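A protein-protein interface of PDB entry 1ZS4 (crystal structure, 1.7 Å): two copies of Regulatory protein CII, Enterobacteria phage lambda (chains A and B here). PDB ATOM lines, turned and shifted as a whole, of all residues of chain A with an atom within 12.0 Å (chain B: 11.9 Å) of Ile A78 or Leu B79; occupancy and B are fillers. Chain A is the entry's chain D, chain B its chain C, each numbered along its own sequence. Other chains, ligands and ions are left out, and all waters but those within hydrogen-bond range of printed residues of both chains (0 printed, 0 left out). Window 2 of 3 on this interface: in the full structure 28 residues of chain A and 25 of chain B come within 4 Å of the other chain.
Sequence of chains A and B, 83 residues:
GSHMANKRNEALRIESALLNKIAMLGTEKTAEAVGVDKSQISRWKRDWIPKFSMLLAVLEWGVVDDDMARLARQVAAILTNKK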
ATOM      1  N   MET A  68      18.032 -17.803 -15.490  1.00  0.00           N
ATOM      2  CA  MET A  68      18.184 -18.205 -14.095  1.00  0.00           C
ATOM      3  C   MET A  68      19.081 -19.436 -13.962  1.00  0.00           C
ATOM      4  O   MET A  68      19.840 -19.557 -12.989  1.00  0.00           O
ATOM      5  CB  MET A  68      16.812 -18.480 -13.456  1.00  0.00           C
ATOM      6  CG  MET A  68      15.904 -17.228 -13.340  1.00  0.00           C
ATOM      7  SD  MET A  68      16.599 -15.824 -12.401  1.00  0.00           S
ATOM      8  CE  MET A  68      17.217 -14.758 -13.710  1.00  0.00           C
ATOM      9  N   ALA A  69      18.997 -20.344 -14.936  1.00  0.00           N
ATOM     10  CA  ALA A  69      19.821 -21.550 -14.911  1.00  0.00           C
ATOM     11  C   ALA A  69      21.285 -21.131 -15.027  1.00  0.00           C
ATOM     12  O   ALA A  69      22.163 -21.698 -14.370  1.00  0.00           O
ATOM     13  CB  ALA A  69      19.425 -22.495 -16.066  1.00  0.00           C
ATOM     14  N   ARG A  70      21.560 -20.181 -15.875  1.00  0.00           N
ATOM     15  CA  ARG A  70      22.889 -19.654 -16.055  1.00  0.00           C
ATOM     16  C   ARG A  70      23.377 -19.013 -14.724  1.00  0.00           C
ATOM     17  O   ARG A  70      24.504 -19.238 -14.273  1.00  0.00           O
ATOM     18  CB  ARG A  70      22.905 -18.644 -17.229  1.00  0.00           C
ATOM     19  CG  ARG A  70      24.306 -18.107 -17.587  1.00  0.00           C
ATOM     20  CD  ARG A  70      24.329 -17.498 -18.984  1.00  0.00           C
ATOM     21  NE  ARG A  70      23.769 -18.430 -19.966  1.00  0.00           N
ATOM     22  CZ  ARG A  70      22.536 -18.319 -20.451  1.00  0.00           C
ATOM     23  NH1 ARG A  70      21.755 -17.342 -20.043  1.00  0.00           N
ATOM     24  NH2 ARG A  70      22.079 -19.190 -21.342  1.00  0.00           N
ATOM     25  N   LEU A  71      22.504 -18.222 -14.106  1.00  0.00           N
ATOM     26  CA  LEU A  71      22.840 -17.575 -12.845  1.00  0.00           C
ATOM     27  C   LEU A  71      23.130 -18.615 -11.769  1.00  0.00           C
ATOM     28  O   LEU A  71      24.090 -18.478 -11.010  1.00  0.00           O
ATOM     29  CB  LEU A  71      21.693 -16.679 -12.358  1.00  0.00           C
ATOM     30  CG  LEU A  71      21.636 -15.228 -12.821  1.00  0.00           C
ATOM     31  CD1 LEU A  71      20.464 -14.541 -12.135  1.00  0.00           C
ATOM     32  CD2 LEU A  71      22.939 -14.518 -12.470  1.00  0.00           C
ATOM     33  N   ALA A  72      22.303 -19.656 -11.706  1.00  0.00           N
ATOM     34  CA  ALA A  72      22.494 -20.690 -10.695  1.00  0.00           C
ATOM     35  C   ALA A  72      23.879 -21.301 -10.849  1.00  0.00           C
ATOM     36  O   ALA A  72      24.582 -21.539  -9.859  1.00  0.00           O
ATOM     37  CB  ALA A  72      21.428 -21.765 -10.821  1.00  0.00           C
ATOM     38  N   ARG A  73      24.276 -21.556 -12.092  1.00  0.00           N
ATOM     39  CA  ARG A  73      25.600 -22.125 -12.328  1.00  0.00           C
ATOM     40  C   ARG A  73      26.702 -21.157 -11.903  1.00  0.00           C
ATOM     41  O   ARG A  73      27.695 -21.576 -11.315  1.00  0.00           O
ATOM     42  CB  ARG A  73      25.779 -22.508 -13.797  1.00  0.00           C
ATOM     43  CG  ARG A  73      24.983 -23.743 -14.226  1.00  0.00           C
ATOM     44  CD  ARG A  73      25.427 -24.229 -15.615  1.00  0.00           C
ATOM     45  NE  ARG A  73      25.051 -23.298 -16.682  1.00  0.00           N
ATOM     46  CZ  ARG A  73      23.860 -23.281 -17.283  1.00  0.00           C
ATOM     47  NH1 ARG A  73      22.920 -24.149 -16.930  1.00  0.00           N
ATOM     48  NH2 ARG A  73      23.602 -22.384 -18.229  1.00  0.00           N
ATOM     49  N   GLN A  74      26.530 -19.864 -12.173  1.00  0.00           N
ATOM     50  CA  GLN A  74      27.562 -18.900 -11.783  1.00  0.00           C
ATOM     51  C   GLN A  74      27.678 -18.826 -10.262  1.00  0.00           C
ATOM     52  O   GLN A  74      28.781 -18.846  -9.710  1.00  0.00           O
ATOM     53  CB  GLN A  74      27.259 -17.512 -12.375  1.00  0.00           C
ATOM     54  CG  GLN A  74      27.176 -17.504 -13.906  1.00  0.00           C
ATOM     55  CD  GLN A  74      26.765 -16.153 -14.469  1.00  0.00           C
ATOM     56  OE1 GLN A  74      25.918 -15.466 -13.899  1.00  0.00           O
ATOM     57  NE2 GLN A  74      27.348 -15.777 -15.605  1.00  0.00           N
ATOM     58  N   VAL A  75      26.536 -18.754  -9.586  1.00  0.00           N
ATOM     59  CA  VAL A  75      26.508 -18.694  -8.123  1.00  0.00           C
ATOM     60  C   VAL A  75      27.082 -19.980  -7.510  1.00  0.00           C
ATOM     61  O   VAL A  75      27.774 -19.942  -6.484  1.00  0.00           O
ATOM     62  CB  VAL A  75      25.059 -18.492  -7.609  1.00  0.00           C
ATOM     63  CG1 VAL A  75      24.999 -18.667  -6.080  1.00  0.00           C
ATOM     64  CG2 VAL A  75      24.568 -17.104  -7.983  1.00  0.00           C
ATOM     65  N   ALA A  76      26.802 -21.116  -8.143  1.00  0.00           N
ATOM     66  CA  ALA A  76      27.305 -22.397  -7.653  1.00  0.00           C
ATOM     67  C   ALA A  76      28.826 -22.376  -7.668  1.00  0.00           C
ATOM     68  O   ALA A  76      29.465 -22.867  -6.739  1.00  0.00           O
ATOM     69  CB  ALA A  76      26.785 -23.548  -8.531  1.00  0.00           C
ATOM     70  N   ALA A  77      29.404 -21.791  -8.713  1.00  0.00           N
ATOM     71  CA  ALA A  77      30.858 -21.724  -8.834  1.00  0.00           C
ATOM     72  C   ALA A  77      31.478 -20.849  -7.746  1.00  0.00           C
ATOM     73  O   ALA A  77      32.594 -21.112  -7.301  1.00  0.00           O
ATOM     74  CB  ALA A  77      31.251 -21.206 -10.209  1.00  0.00           C
ATOM     75  N   ILE A  78      30.755 -19.816  -7.320  1.00  0.00           N
ATOM     76  CA  ILE A  78      31.236 -18.915  -6.269  1.00  0.00           C
ATOM     77  C   ILE A  78      31.176 -19.596  -4.904  1.00  0.00           C
ATOM     78  O   ILE A  78      32.146 -19.584  -4.140  1.00  0.00           O
ATOM     79  CB  ILE A  78      30.371 -17.626  -6.164  1.00  0.00           C
ATOM     80  CG1 ILE A  78      30.347 -16.875  -7.497  1.00  0.00           C
ATOM     81  CG2 ILE A  78      30.924 -16.723  -5.066  1.00  0.00           C
ATOM     82  CD1 ILE A  78      31.709 -16.595  -8.051  1.00  0.00           C
ATOM     83  N   LEU A  79      30.022 -20.179  -4.599  1.00  0.00           N
ATOM     84  CA  LEU A  79      29.801 -20.841  -3.322  1.00  0.00           C
ATOM     85  C   LEU A  79      30.554 -22.154  -3.127  1.00  0.00           C
ATOM     86  O   LEU A  79      30.787 -22.575  -1.991  1.00  0.00           O
ATOM     87  CB  LEU A  79      28.307 -21.086  -3.119  1.00  0.00           C
ATOM     88  CG  LEU A  79      27.434 -19.834  -3.048  1.00  0.00           C
ATOM     89  CD1 LEU A  79      25.991 -20.249  -2.780  1.00  0.00           C
ATOM     90  CD2 LEU A  79      27.935 -18.911  -1.948  1.00  0.00           C
ATOM     91  N   THR A  80      30.922 -22.806  -4.224  1.00  0.00           N
ATOM     92  CA  THR A  80      31.644 -24.069  -4.133  1.00  0.00           C
ATOM     93  C   THR A  80      33.019 -23.848  -3.519  1.00  0.00           C
ATOM     94  O   THR A  80      33.315 -24.514  -2.499  1.00  0.00           O
ATOM     95  CB  THR A  80      31.803 -24.728  -5.522  1.00  0.00           C
ATOM     96  OG1 THR A  80      30.531 -25.218  -5.961  1.00  0.00           O
ATOM     97  CG2 THR A  80      32.777 -25.884  -5.460  1.00  0.00           C
ATOM     98  N   ARG B  70      13.607 -11.286 -10.427  1.00  0.00           N
ATOM     99  CA  ARG B  70      14.312 -10.039 -10.128  1.00  0.00           C
ATOM    100  C   ARG B  70      15.102 -10.204  -8.839  1.00  0.00           C
ATOM    101  O   ARG B  70      16.274  -9.829  -8.770  1.00  0.00           O
ATOM    102  CB  ARG B  70      13.355  -8.867  -9.921  1.00  0.00           C
ATOM    103  CG  ARG B  70      14.113  -7.617  -9.507  1.00  0.00           C
ATOM    104  CD  ARG B  70      13.259  -6.557  -8.845  1.00  0.00           C
ATOM    105  NE  ARG B  70      14.128  -5.479  -8.379  1.00  0.00           N
ATOM    106  CZ  ARG B  70      14.740  -4.618  -9.187  1.00  0.00           C
ATOM    107  NH1 ARG B  70      14.570  -4.689 -10.504  1.00  0.00           N
ATOM    108  NH2 ARG B  70      15.555  -3.702  -8.676  1.00  0.00           N
ATOM    109  N   LEU B  71      14.443 -10.740  -7.821  1.00  0.00           N
ATOM    110  CA  LEU B  71      15.082 -10.956  -6.526  1.00  0.00           C
ATOM    111  C   LEU B  71      16.257 -11.916  -6.656  1.00  0.00           C
ATOM    112  O   LEU B  71      17.281 -11.737  -6.000  1.00  0.00           O
ATOM    113  CB  LEU B  71      14.076 -11.501  -5.511  1.00  0.00           C
ATOM    114  CG  LEU B  71      13.012 -10.500  -5.044  1.00  0.00           C
ATOM    115  CD1 LEU B  71      12.046 -11.186  -4.073  1.00  0.00           C
ATOM    116  CD2 LEU B  71      13.695  -9.294  -4.391  1.00  0.00           C
ATOM    117  N   ALA B  72      16.107 -12.929  -7.508  1.00  0.00           N
ATOM    118  CA  ALA B  72      17.175 -13.908  -7.719  1.00  0.00           C
ATOM    119  C   ALA B  72      18.375 -13.212  -8.350  1.00  0.00           C
ATOM    120  O   ALA B  72      19.521 -13.487  -8.005  1.00  0.00           O
ATOM    121  CB  ALA B  72      16.673 -15.049  -8.616  1.00  0.00           C
ATOM    122  N   ARG B  73      18.122 -12.308  -9.291  1.00  0.00           N
ATOM    123  CA  ARG B  73      19.227 -11.591  -9.913  1.00  0.00           C
ATOM    124  C   ARG B  73      19.943 -10.711  -8.889  1.00  0.00           C
ATOM    125  O   ARG B  73      21.174 -10.640  -8.873  1.00  0.00           O
ATOM    126  CB  ARG B  73      18.721 -10.740 -11.087  1.00  0.00           C
ATOM    127  CG  ARG B  73      18.088 -11.501 -12.247  1.00  0.00           C
ATOM    128  CD  ARG B  73      17.256 -10.552 -13.108  1.00  0.00           C
ATOM    129  NE  ARG B  73      16.851 -11.117 -14.400  1.00  0.00           N
ATOM    130  CZ  ARG B  73      17.689 -11.527 -15.371  1.00  0.00           C
ATOM    131  NH1 ARG B  73      19.003 -11.424 -15.191  1.00  0.00           N
ATOM    132  NH2 ARG B  73      17.193 -12.025 -16.504  1.00  0.00           N
ATOM    133  N   GLN B  74      19.168 -10.030  -8.051  1.00  0.00           N
ATOM    134  CA  GLN B  74      19.730  -9.139  -7.035  1.00  0.00           C
ATOM    135  C   GLN B  74      20.567  -9.944  -6.054  1.00  0.00           C
ATOM    136  O   GLN B  74      21.682  -9.556  -5.714  1.00  0.00           O
ATOM    137  CB  GLN B  74      18.605  -8.409  -6.295  1.00  0.00           C
ATOM    138  CG  GLN B  74      17.792  -7.460  -7.173  1.00  0.00           C
ATOM    139  CD  GLN B  74      18.470  -6.123  -7.425  1.00  0.00           C
ATOM    140  OE1 GLN B  74      18.459  -5.617  -8.549  1.00  0.00           O
ATOM    141  NE2 GLN B  74      19.051  -5.539  -6.387  1.00  0.00           N
ATOM    142  N   VAL B  75      20.015 -11.060  -5.597  1.00  0.00           N
ATOM    143  CA  VAL B  75      20.716 -11.936  -4.661  1.00  0.00           C
ATOM    144  C   VAL B  75      22.007 -12.479  -5.276  1.00  0.00           C
ATOM    145  O   VAL B  75      23.063 -12.486  -4.629  1.00  0.00           O
ATOM    146  CB  VAL B  75      19.807 -13.119  -4.233  1.00  0.00           C
ATOM    147  CG1 VAL B  75      20.626 -14.185  -3.512  1.00  0.00           C
ATOM    148  CG2 VAL B  75      18.673 -12.602  -3.325  1.00  0.00           C
ATOM    149  N   ALA B  76      21.936 -12.933  -6.522  1.00  0.00           N
ATOM    150  CA  ALA B  76      23.129 -13.464  -7.180  1.00  0.00           C
ATOM    151  C   ALA B  76      24.216 -12.389  -7.242  1.00  0.00           C
ATOM    152  O   ALA B  76      25.396 -12.685  -7.026  1.00  0.00           O
ATOM    153  CB  ALA B  76      22.792 -13.979  -8.595  1.00  0.00           C
ATOM    154  N   ALA B  77      23.833 -11.140  -7.522  1.00  0.00           N
ATOM    155  CA  ALA B  77      24.822 -10.060  -7.571  1.00  0.00           C
ATOM    156  C   ALA B  77      25.498  -9.900  -6.203  1.00  0.00           C
ATOM    157  O   ALA B  77      26.713  -9.717  -6.125  1.00  0.00           O
ATOM    158  CB  ALA B  77      24.160  -8.749  -7.971  1.00  0.00           C
ATOM    159  N   ILE B  78      24.703  -9.966  -5.139  1.00  0.00           N
ATOM    160  CA  ILE B  78      25.199  -9.844  -3.777  1.00  0.00           C
ATOM    161  C   ILE B  78      26.142 -10.997  -3.444  1.00  0.00           C
ATOM    162  O   ILE B  78      27.231 -10.780  -2.929  1.00  0.00           O
ATOM    163  CB  ILE B  78      24.024  -9.802  -2.756  1.00  0.00           C
ATOM    164  CG1 ILE B  78      23.239  -8.494  -2.950  1.00  0.00           C
ATOM    165  CG2 ILE B  78      24.550  -9.909  -1.317  1.00  0.00           C
ATOM    166  CD1 ILE B  78      21.941  -8.421  -2.168  1.00  0.00           C
ATOM    167  N   LEU B  79      25.744 -12.220  -3.769  1.00  0.00           N
ATOM    168  CA  LEU B  79      26.586 -13.369  -3.470  1.00  0.00           C
ATOM    169  C   LEU B  79      27.883 -13.332  -4.255  1.00  0.00           C
ATOM    170  O   LEU B  79      28.929 -13.753  -3.762  1.00  0.00           O
ATOM    171  CB  LEU B  79      25.830 -14.671  -3.770  1.00  0.00           C
ATOM    172  CG  LEU B  79      24.568 -14.880  -2.929  1.00  0.00           C
ATOM    173  CD1 LEU B  79      24.059 -16.293  -3.147  1.00  0.00           C
ATOM    174  CD2 LEU B  79      24.870 -14.635  -1.445  1.00  0.00           C
ATOM    175  N   THR B  80      27.819 -12.803  -5.471  1.00  0.00           N
ATOM    176  CA  THR B  80      28.980 -12.729  -6.340  1.00  0.00           C
ATOM    177  C   THR B  80      29.956 -11.593  -6.020  1.00  0.00           C
ATOM    178  O   THR B  80      31.180 -11.795  -6.010  1.00  0.00           O
ATOM    179  CB  THR B  80      28.539 -12.569  -7.801  1.00  0.00           C
ATOM    180  OG1 THR B  80      27.775 -13.714  -8.198  1.00  0.00           O
ATOM    181  CG2 THR B  80      29.739 -12.429  -8.708  1.00  0.00           C
ATOM    182  N   ASN B  81      29.416 -10.409  -5.747  1.00  0.00           N
ATOM    183  CA  ASN B  81      30.250  -9.236  -5.501  1.00  0.00           C
ATOM    184  C   ASN B  81      30.367  -8.681  -4.081  1.00  0.00           C
ATOM    185  O   ASN B  81      31.232  -7.842  -3.835  1.00  0.00           O
ATOM    186  CB  ASN B  81      29.795  -8.103  -6.427  1.00  0.00           C
ATOM    187  CG  ASN B  81      29.998  -8.428  -7.896  1.00  0.00           C
ATOM    188  OD1 ASN B  81      29.378  -7.812  -8.773  1.00  0.00           O
ATOM    189  ND2 ASN B  81      30.875  -9.383  -8.176  1.00  0.00           N
ATOM    190  N   LYS B  82      29.514  -9.110  -3.157  1.00  0.00           N
ATOM    191  CA  LYS B  82      29.587  -8.590  -1.791  1.00  0.00           C
ATOM    192  C   LYS B  82      30.626  -9.320  -0.944  1.00  0.00           C
ATOM    193  O   LYS B  82      30.593 -10.544  -0.824  1.00  0.00           O
ATOM    194  CB  LYS B  82      28.221  -8.676  -1.103  1.00  0.00           C
ATOM    195  CG  LYS B  82      28.273  -8.451   0.406  1.00  0.00           C
ATOM    196  CD  LYS B  82      26.904  -8.646   1.047  1.00  0.00           C
ATOM    197  CE  LYS B  82      27.025  -8.864   2.547  1.00  0.00           C
ATOM    198  NZ  LYS B  82      27.839  -7.803   3.209  1.00  0.00           N
ATOM    199  N   LYS B  83      31.534  -8.552  -0.348  1.00  0.00           N
ATOM    200  CA  LYS B  83      32.593  -9.111   0.486  1.00  0.00           C
ATOM    201  C   LYS B  83      32.614  -8.496   1.886  1.00  0.00           C
ATOM    202  O   LYS B  83      33.460  -7.601   2.120  1.00  0.00           O
ATOM    203  CB  LYS B  83      33.951  -8.908  -0.185  1.00  0.00           C
ATOM    204  CG  LYS B  83      34.213  -7.480  -0.635  1.00  0.00           C
ATOM    205  CD  LYS B  83      35.688  -7.264  -0.912  1.00  0.00           C
ATOM    206  CE  LYS B  83      36.227  -8.335  -1.845  1.00  0.00           C
ATOM    207  NZ  LYS B  83      35.545  -8.322  -3.170  1.00  0.00           N
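Among the printed residues, merely in contact across the chains: Met A68 with Ala B72 (3.9 Å), Met A68 with Arg B73 (3.7 Å), Leu A71 with Arg B73 (3.9 Å), Leu A71 with Ala B76 (3.9 Å), Val A75 with Ala B76 (3.6 Å), Val A75 with Leu B79 (3.9 Å) and Ile A78 with Leu B79 (3.8 Å).
Leu A71 touches Arg B73, but with the chains exchanged Arg A73 does not touch Leu B71 (13.5 Å).
Leu A71 touches Ala B76, but with the chains exchanged Ala A76 does not touch Leu B71 (13.5 Å).
Val A75 touches Ala B76, but with the chains exchanged Ala A76 does not touch Val B75 (10.0 Å).
Val A75 touches Leu B79, but with the chains exchanged Leu A79 does not touch Val B75 (8.1 Å).
Positions printed for both chains: 70, 71, 72, 73, 74, 75, 76, 77, 78, 79 and 80.
Of the 7 pairs that touch across the chains among the printed residues, none has its exchanged pair printed and touching as well.
OG1 of Thr B80 lies within hydrogen-bond range of O of Ala B76, at 2.8 Å.
Hydrophobic or aromatic side chains of chain B within 4 Å of the printed part of chain A: Ala B72, Ala B76 and Leu B79.
Of the 13 printed residues of chain A, 4 touch a printed residue of chain B.
Of chain B, only Leu B79 comes within 4 Å of Ile A78.
No residue of chain B comes within 4 Å of Ala A77.
Of chain A, only Leu A71 and Val A75 come within 4 Å of Ala B76.
Of the printed residues of chain A, Ala B72 touches Met A68 (3.9 Å).
Of the printed residues of chain B, Leu A71 touches Arg B73 and Ala B76.
Of the printed residues of chain B, Met A68 touches Ala B72 and Arg B73.
Of the printed residues of chain A, Arg B73 touches Met A68 (3.7 Å) and Leu A71 (3.9 Å).
The nearest printed residue of chain A that does not touch Ala B72 is Leu A71 (4.4 Å).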
